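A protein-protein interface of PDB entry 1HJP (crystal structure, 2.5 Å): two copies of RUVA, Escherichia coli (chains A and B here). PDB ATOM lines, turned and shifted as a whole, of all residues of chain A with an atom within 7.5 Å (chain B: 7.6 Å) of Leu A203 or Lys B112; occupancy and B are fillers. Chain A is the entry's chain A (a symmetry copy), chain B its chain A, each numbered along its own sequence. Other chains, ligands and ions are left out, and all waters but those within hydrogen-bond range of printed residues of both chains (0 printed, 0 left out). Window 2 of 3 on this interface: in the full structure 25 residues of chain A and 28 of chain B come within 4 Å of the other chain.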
ATOM      1  N   TYR A 172     -33.768 -15.009   5.622  1.00  0.00           N
ATOM      2  CA  TYR A 172     -32.634 -14.720   4.752  1.00  0.00           C
ATOM      3  C   TYR A 172     -32.951 -13.452   3.948  1.00  0.00           C
ATOM      4  O   TYR A 172     -34.121 -13.124   3.703  1.00  0.00           O
ATOM      5  CB  TYR A 172     -32.352 -15.858   3.778  1.00  0.00           C
ATOM      6  CG  TYR A 172     -31.766 -17.097   4.411  1.00  0.00           C
ATOM      7  CD1 TYR A 172     -30.549 -17.054   5.080  1.00  0.00           C
ATOM      8  CD2 TYR A 172     -32.439 -18.314   4.343  1.00  0.00           C
ATOM      9  CE1 TYR A 172     -30.018 -18.189   5.661  1.00  0.00           C
ATOM     10  CE2 TYR A 172     -31.916 -19.454   4.924  1.00  0.00           C
ATOM     11  CZ  TYR A 172     -30.707 -19.382   5.581  1.00  0.00           C
ATOM     12  OH  TYR A 172     -30.175 -20.508   6.163  1.00  0.00           O
ATOM     13  N   GLU A 176     -29.156 -13.100  -0.769  1.00  0.00           N
ATOM     14  CA  GLU A 176     -28.522 -14.300  -0.237  1.00  0.00           C
ATOM     15  C   GLU A 176     -29.402 -15.524  -0.445  1.00  0.00           C
ATOM     16  O   GLU A 176     -28.887 -16.618  -0.681  1.00  0.00           O
ATOM     17  CB  GLU A 176     -28.096 -14.129   1.215  1.00  0.00           C
ATOM     18  CG  GLU A 176     -29.170 -13.938   2.255  1.00  0.00           C
ATOM     19  CD  GLU A 176     -28.688 -13.382   3.579  1.00  0.00           C
ATOM     20  OE1 GLU A 176     -28.177 -12.241   3.618  1.00  0.00           O
ATOM     21  OE2 GLU A 176     -28.817 -14.076   4.612  1.00  0.00           O
ATOM     22  N   ALA A 198     -31.405 -26.408  -0.288  1.00  0.00           N
ATOM     23  CA  ALA A 198     -30.756 -25.134  -0.024  1.00  0.00           C
ATOM     24  C   ALA A 198     -30.463 -24.876   1.447  1.00  0.00           C
ATOM     25  O   ALA A 198     -29.487 -24.226   1.825  1.00  0.00           O
ATOM     26  CB  ALA A 198     -31.621 -23.999  -0.579  1.00  0.00           C
ATOM     27  N   LEU A 199     -31.339 -25.358   2.318  1.00  0.00           N
ATOM     28  CA  LEU A 199     -31.202 -25.175   3.759  1.00  0.00           C
ATOM     29  C   LEU A 199     -30.171 -26.148   4.316  1.00  0.00           C
ATOM     30  O   LEU A 199     -29.443 -25.824   5.253  1.00  0.00           O
ATOM     31  CB  LEU A 199     -32.560 -25.341   4.418  1.00  0.00           C
ATOM     32  CG  LEU A 199     -33.094 -24.327   5.417  1.00  0.00           C
ATOM     33  CD1 LEU A 199     -32.412 -22.973   5.345  1.00  0.00           C
ATOM     34  CD2 LEU A 199     -34.599 -24.171   5.227  1.00  0.00           C
ATOM     35  N   ARG A 200     -30.092 -27.325   3.701  1.00  0.00           N
ATOM     36  CA  ARG A 200     -29.155 -28.367   4.098  1.00  0.00           C
ATOM     37  C   ARG A 200     -27.701 -27.963   3.869  1.00  0.00           C
ATOM     38  O   ARG A 200     -26.830 -28.181   4.711  1.00  0.00           O
ATOM     39  CB  ARG A 200     -29.466 -29.653   3.333  1.00  0.00           C
ATOM     40  CG  ARG A 200     -28.700 -30.883   3.790  1.00  0.00           C
ATOM     41  CD  ARG A 200     -29.529 -32.143   3.556  1.00  0.00           C
ATOM     42  NE  ARG A 200     -30.828 -32.037   4.200  1.00  0.00           N
ATOM     43  CZ  ARG A 200     -31.800 -32.933   4.252  1.00  0.00           C
ATOM     44  NH1 ARG A 200     -31.682 -34.120   3.671  1.00  0.00           N
ATOM     45  NH2 ARG A 200     -32.928 -32.639   4.897  1.00  0.00           N
ATOM     46  N   ALA A 201     -27.441 -27.325   2.734  1.00  0.00           N
ATOM     47  CA  ALA A 201     -26.119 -26.858   2.358  1.00  0.00           C
ATOM     48  C   ALA A 201     -25.889 -25.403   2.746  1.00  0.00           C
ATOM     49  O   ALA A 201     -25.458 -24.582   1.934  1.00  0.00           O
ATOM     50  CB  ALA A 201     -25.942 -27.041   0.852  1.00  0.00           C
ATOM     51  N   ALA A 202     -26.167 -25.067   3.997  1.00  0.00           N
ATOM     52  CA  ALA A 202     -25.993 -23.723   4.524  1.00  0.00           C
ATOM     53  C   ALA A 202     -25.927 -23.782   6.048  1.00  0.00           C
ATOM     54  O   ALA A 202     -25.685 -22.789   6.723  1.00  0.00           O
ATOM     55  CB  ALA A 202     -27.112 -22.803   4.075  1.00  0.00           C
ATOM     56  N   LEU A 203     -26.168 -24.975   6.582  1.00  0.00           N
ATOM     57  CA  LEU A 203     -26.128 -25.224   8.015  1.00  0.00           C
ATOM     58  C   LEU A 203     -25.207 -26.411   8.317  1.00  0.00           C
ATOM     59  O   LEU A 203     -24.068 -26.179   8.779  1.00  0.00           O
ATOM     60  CB  LEU A 203     -27.520 -25.495   8.583  1.00  0.00           C
ATOM     61  CG  LEU A 203     -28.612 -24.447   8.368  1.00  0.00           C
ATOM     62  CD1 LEU A 203     -29.971 -24.973   8.797  1.00  0.00           C
ATOM     63  CD2 LEU A 203     -28.286 -23.155   9.104  1.00  0.00           C
ATOM     64  OXT LEU A 203     -25.500 -27.526   7.824  1.00  0.00           O
ATOM     65  N   ALA B  88     -37.909 -20.483  11.781  1.00  0.00           N
ATOM     66  CA  ALA B  88     -36.663 -20.727  11.065  1.00  0.00           C
ATOM     67  C   ALA B  88     -35.831 -21.827  11.728  1.00  0.00           C
ATOM     68  O   ALA B  88     -35.290 -22.690  11.021  1.00  0.00           O
ATOM     69  CB  ALA B  88     -35.853 -19.448  10.951  1.00  0.00           C
ATOM     70  N   ILE B  89     -35.772 -21.845  13.062  1.00  0.00           N
ATOM     71  CA  ILE B  89     -35.034 -22.902  13.748  1.00  0.00           C
ATOM     72  C   ILE B  89     -35.608 -24.271  13.403  1.00  0.00           C
ATOM     73  O   ILE B  89     -34.874 -25.178  12.973  1.00  0.00           O
ATOM     74  CB  ILE B  89     -34.997 -22.723  15.266  1.00  0.00           C
ATOM     75  CG1 ILE B  89     -34.299 -21.411  15.642  1.00  0.00           C
ATOM     76  CG2 ILE B  89     -34.315 -23.923  15.910  1.00  0.00           C
ATOM     77  CD1 ILE B  89     -34.435 -21.059  17.110  1.00  0.00           C
ATOM     78  N   SER B  91     -37.107 -25.055  10.783  1.00  0.00           N
ATOM     79  CA  SER B  91     -37.097 -25.210   9.335  1.00  0.00           C
ATOM     80  C   SER B  91     -35.740 -25.790   8.938  1.00  0.00           C
ATOM     81  O   SER B  91     -35.612 -26.692   8.127  1.00  0.00           O
ATOM     82  CB  SER B  91     -37.284 -23.883   8.611  1.00  0.00           C
ATOM     83  OG  SER B  91     -38.665 -23.562   8.551  1.00  0.00           O
ATOM     84  N   GLY B  92     -34.729 -25.249   9.623  1.00  0.00           N
ATOM     85  CA  GLY B  92     -33.348 -25.648   9.422  1.00  0.00           C
ATOM     86  C   GLY B  92     -33.099 -27.033  10.000  1.00  0.00           C
ATOM     87  O   GLY B  92     -32.251 -27.767   9.471  1.00  0.00           O
ATOM     88  N   MET B  93     -33.799 -27.398  11.064  1.00  0.00           N
ATOM     89  CA  MET B  93     -33.593 -28.730  11.626  1.00  0.00           C
ATOM     90  C   MET B  93     -34.878 -29.274  12.230  1.00  0.00           C
ATOM     91  O   MET B  93     -35.801 -28.529  12.565  1.00  0.00           O
ATOM     92  CB  MET B  93     -32.426 -28.763  12.595  1.00  0.00           C
ATOM     93  CG  MET B  93     -32.429 -27.917  13.837  1.00  0.00           C
ATOM     94  SD  MET B  93     -30.770 -27.659  14.523  1.00  0.00           S
ATOM     95  CE  MET B  93     -30.932 -25.962  15.075  1.00  0.00           C
ATOM     96  N   VAL B 107     -23.459 -25.176  19.864  1.00  0.00           N
ATOM     97  CA  VAL B 107     -23.701 -23.768  19.593  1.00  0.00           C
ATOM     98  C   VAL B 107     -22.825 -23.309  18.438  1.00  0.00           C
ATOM     99  O   VAL B 107     -21.983 -22.416  18.510  1.00  0.00           O
ATOM    100  CB  VAL B 107     -23.463 -22.942  20.865  1.00  0.00           C
ATOM    101  CG1 VAL B 107     -22.063 -23.176  21.419  1.00  0.00           C
ATOM    102  CG2 VAL B 107     -23.719 -21.459  20.642  1.00  0.00           C
ATOM    103  N   GLY B 108     -23.003 -23.987  17.313  1.00  0.00           N
ATOM    104  CA  GLY B 108     -22.274 -23.742  16.073  1.00  0.00           C
ATOM    105  C   GLY B 108     -23.215 -24.183  14.943  1.00  0.00           C
ATOM    106  O   GLY B 108     -23.212 -23.702  13.820  1.00  0.00           O
ATOM    107  N   ALA B 109     -24.097 -25.097  15.343  1.00  0.00           N
ATOM    108  CA  ALA B 109     -25.137 -25.635  14.486  1.00  0.00           C
ATOM    109  C   ALA B 109     -26.274 -24.627  14.336  1.00  0.00           C
ATOM    110  O   ALA B 109     -26.963 -24.601  13.325  1.00  0.00           O
ATOM    111  CB  ALA B 109     -25.682 -26.912  15.120  1.00  0.00           C
ATOM    112  N   LEU B 110     -26.471 -23.811  15.363  1.00  0.00           N
ATOM    113  CA  LEU B 110     -27.535 -22.832  15.407  1.00  0.00           C
ATOM    114  C   LEU B 110     -27.115 -21.436  14.984  1.00  0.00           C
ATOM    115  O   LEU B 110     -27.942 -20.616  14.597  1.00  0.00           O
ATOM    116  CB  LEU B 110     -28.049 -22.727  16.853  1.00  0.00           C
ATOM    117  CG  LEU B 110     -29.039 -23.807  17.290  1.00  0.00           C
ATOM    118  CD1 LEU B 110     -28.776 -24.194  18.734  1.00  0.00           C
ATOM    119  CD2 LEU B 110     -30.452 -23.285  17.088  1.00  0.00           C
ATOM    120  N   VAL B 111     -25.825 -21.155  15.064  1.00  0.00           N
ATOM    121  CA  VAL B 111     -25.272 -19.845  14.749  1.00  0.00           C
ATOM    122  C   VAL B 111     -25.435 -19.474  13.287  1.00  0.00           C
ATOM    123  O   VAL B 111     -25.563 -18.290  12.958  1.00  0.00           O
ATOM    124  CB  VAL B 111     -23.808 -19.741  15.221  1.00  0.00           C
ATOM    125  CG1 VAL B 111     -22.852 -20.507  14.321  1.00  0.00           C
ATOM    126  CG2 VAL B 111     -23.396 -18.281  15.332  1.00  0.00           C
ATOM    127  N   LYS B 112     -25.491 -20.456  12.401  1.00  0.00           N
ATOM    128  CA  LYS B 112     -25.683 -20.229  10.981  1.00  0.00           C
ATOM    129  C   LYS B 112     -27.059 -19.642  10.660  1.00  0.00           C
ATOM    130  O   LYS B 112     -27.188 -18.721   9.847  1.00  0.00           O
ATOM    131  CB  LYS B 112     -25.473 -21.530  10.203  1.00  0.00           C
ATOM    132  CG  LYS B 112     -25.214 -22.768  11.036  1.00  0.00           C
ATOM    133  CD  LYS B 112     -23.980 -23.538  10.607  1.00  0.00           C
ATOM    134  CE  LYS B 112     -22.697 -22.730  10.654  1.00  0.00           C
ATOM    135  NZ  LYS B 112     -21.751 -23.174  11.711  1.00  0.00           N
ATOM    136  N   LEU B 113     -28.104 -20.182  11.283  1.00  0.00           N
ATOM    137  CA  LEU B 113     -29.471 -19.729  11.067  1.00  0.00           C
ATOM    138  C   LEU B 113     -29.614 -18.234  11.297  1.00  0.00           C
ATOM    139  O   LEU B 113     -29.098 -17.667  12.259  1.00  0.00           O
ATOM    140  CB  LEU B 113     -30.432 -20.555  11.932  1.00  0.00           C
ATOM    141  CG  LEU B 113     -30.550 -22.001  11.411  1.00  0.00           C
ATOM    142  CD1 LEU B 113     -30.363 -23.017  12.520  1.00  0.00           C
ATOM    143  CD2 LEU B 113     -31.873 -22.176  10.683  1.00  0.00           C
ATOM    144  N   PRO B 114     -30.302 -17.565  10.370  1.00  0.00           N
ATOM    145  CA  PRO B 114     -30.455 -16.133  10.383  1.00  0.00           C
ATOM    146  C   PRO B 114     -31.284 -15.543  11.504  1.00  0.00           C
ATOM    147  O   PRO B 114     -32.301 -16.102  11.901  1.00  0.00           O
ATOM    148  CB  PRO B 114     -31.117 -15.803   9.046  1.00  0.00           C
ATOM    149  CG  PRO B 114     -31.716 -17.070   8.566  1.00  0.00           C
ATOM    150  CD  PRO B 114     -30.911 -18.188   9.164  1.00  0.00           C
ATOM    151  N   GLY B 115     -30.874 -14.372  11.980  1.00  0.00           N
ATOM    152  CA  GLY B 115     -31.600 -13.616  12.963  1.00  0.00           C
ATOM    153  C   GLY B 115     -31.290 -13.843  14.420  1.00  0.00           C
ATOM    154  O   GLY B 115     -31.916 -13.166  15.255  1.00  0.00           O
ATOM    155  N   ILE B 116     -30.372 -14.749  14.751  1.00  0.00           N
ATOM    156  CA  ILE B 116     -30.097 -14.987  16.173  1.00  0.00           C
ATOM    157  C   ILE B 116     -28.726 -14.517  16.612  1.00  0.00           C
ATOM    158  O   ILE B 116     -28.656 -13.592  17.436  1.00  0.00           O
ATOM    159  CB  ILE B 116     -30.404 -16.451  16.537  1.00  0.00           C
ATOM    160  CG1 ILE B 116     -30.224 -16.665  18.043  1.00  0.00           C
ATOM    161  CG2 ILE B 116     -29.588 -17.441  15.719  1.00  0.00           C
ATOM    162  CD1 ILE B 116     -30.954 -17.876  18.578  1.00  0.00           C
ATOM    163  N   GLY B 117     -27.626 -15.079  16.124  1.00  0.00           N
ATOM    164  CA  GLY B 117     -26.305 -14.631  16.544  1.00  0.00           C
ATOM    165  C   GLY B 117     -25.503 -15.678  17.300  1.00  0.00           C
ATOM    166  O   GLY B 117     -25.629 -16.878  17.050  1.00  0.00           O
ATOM    167  N   LYS B 118     -24.631 -15.224  18.202  1.00  0.00           N
ATOM    168  CA  LYS B 118     -23.778 -16.124  18.968  1.00  0.00           C
ATOM    169  C   LYS B 118     -24.146 -16.163  20.446  1.00  0.00           C
ATOM    170  O   LYS B 118     -24.276 -17.245  21.020  1.00  0.00           O
ATOM    171  CB  LYS B 118     -22.303 -15.766  18.802  1.00  0.00           C
ATOM    172  CG  LYS B 118     -21.858 -15.459  17.383  1.00  0.00           C
ATOM    173  CD  LYS B 118     -22.061 -13.990  17.030  1.00  0.00           C
ATOM    174  CE  LYS B 118     -22.341 -13.766  15.559  1.00  0.00           C
ATOM    175  NZ  LYS B 118     -23.134 -14.859  14.935  1.00  0.00           N
ATOM    176  N   ALA B 121     -27.616 -17.698  20.721  1.00  0.00           N
ATOM    177  CA  ALA B 121     -27.479 -19.130  20.495  1.00  0.00           C
ATOM    178  C   ALA B 121     -27.092 -19.808  21.815  1.00  0.00           C
ATOM    179  O   ALA B 121     -27.736 -20.745  22.284  1.00  0.00           O
ATOM    180  CB  ALA B 121     -26.418 -19.409  19.445  1.00  0.00           C
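O of Gly B108 is in hydrogen-bond range of NZ of Lys B112, 2.6 Å away.
Among the printed residues, merely in contact across the chains: Leu A203 with Lys B112 (3.2 Å), Leu A203 with Leu B113 (3.4 Å), Leu A203 with Gly B92 (3.5 Å), Tyr A172 with Pro B114 (3.5 Å), Ala A202 with Lys B112 (3.7 Å) and Leu A199 with Ser B91 (3.97 Å).
Leu A203 touches just these residues of chain B: Gly B92 (3.5 Å), Lys B112 (3.2 Å) and Leu B113 (3.4 Å).
Lys B112 touches just these residues of chain A: Ala A202 (3.7 Å) and Leu A203 (3.2 Å).
Of chain B, only Lys B112 comes within 4 Å of Ala A202.
Printed residues of chain A within 4 Å of Leu B113: Leu A203 (3.4 Å).
Of the printed residues of chain B, Tyr A172 touches Pro B114.
Printed residues of chain A within 4 Å of Ser B91: Leu A199.
Printed residues of chain A within 4 Å of Gly B92: Leu A203 (3.5 Å).
Ala B109 touches none of the printed residues of chain A.
Val B111 touches none of the printed residues of chain A.
The nearest residue of chain B that does not touch Leu A203 is Ala B109 (4.7 Å).
The nearest residue of chain A that does not touch Lys B112 is Tyr A172 (5.1 Å).
The nearest printed residue of chain A that does not touch Gly B92 is Leu A199 (4.2 Å).
Printed residues of chain B that touch a printed residue of chain A: Ser B91, Gly B92, Lys B112, Leu B113 and Pro B114.
Hydrophobic or aromatic side chains of chain B within 4 Å of the printed part of chain A: Leu B113 and Pro B114.
Among the printed residues, 6 pairs touch across the chains.
No position is printed for both chains.
Of the 6 pairs that touch across the chains among the printed residues, none has its exchanged pair printed and touching as well.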
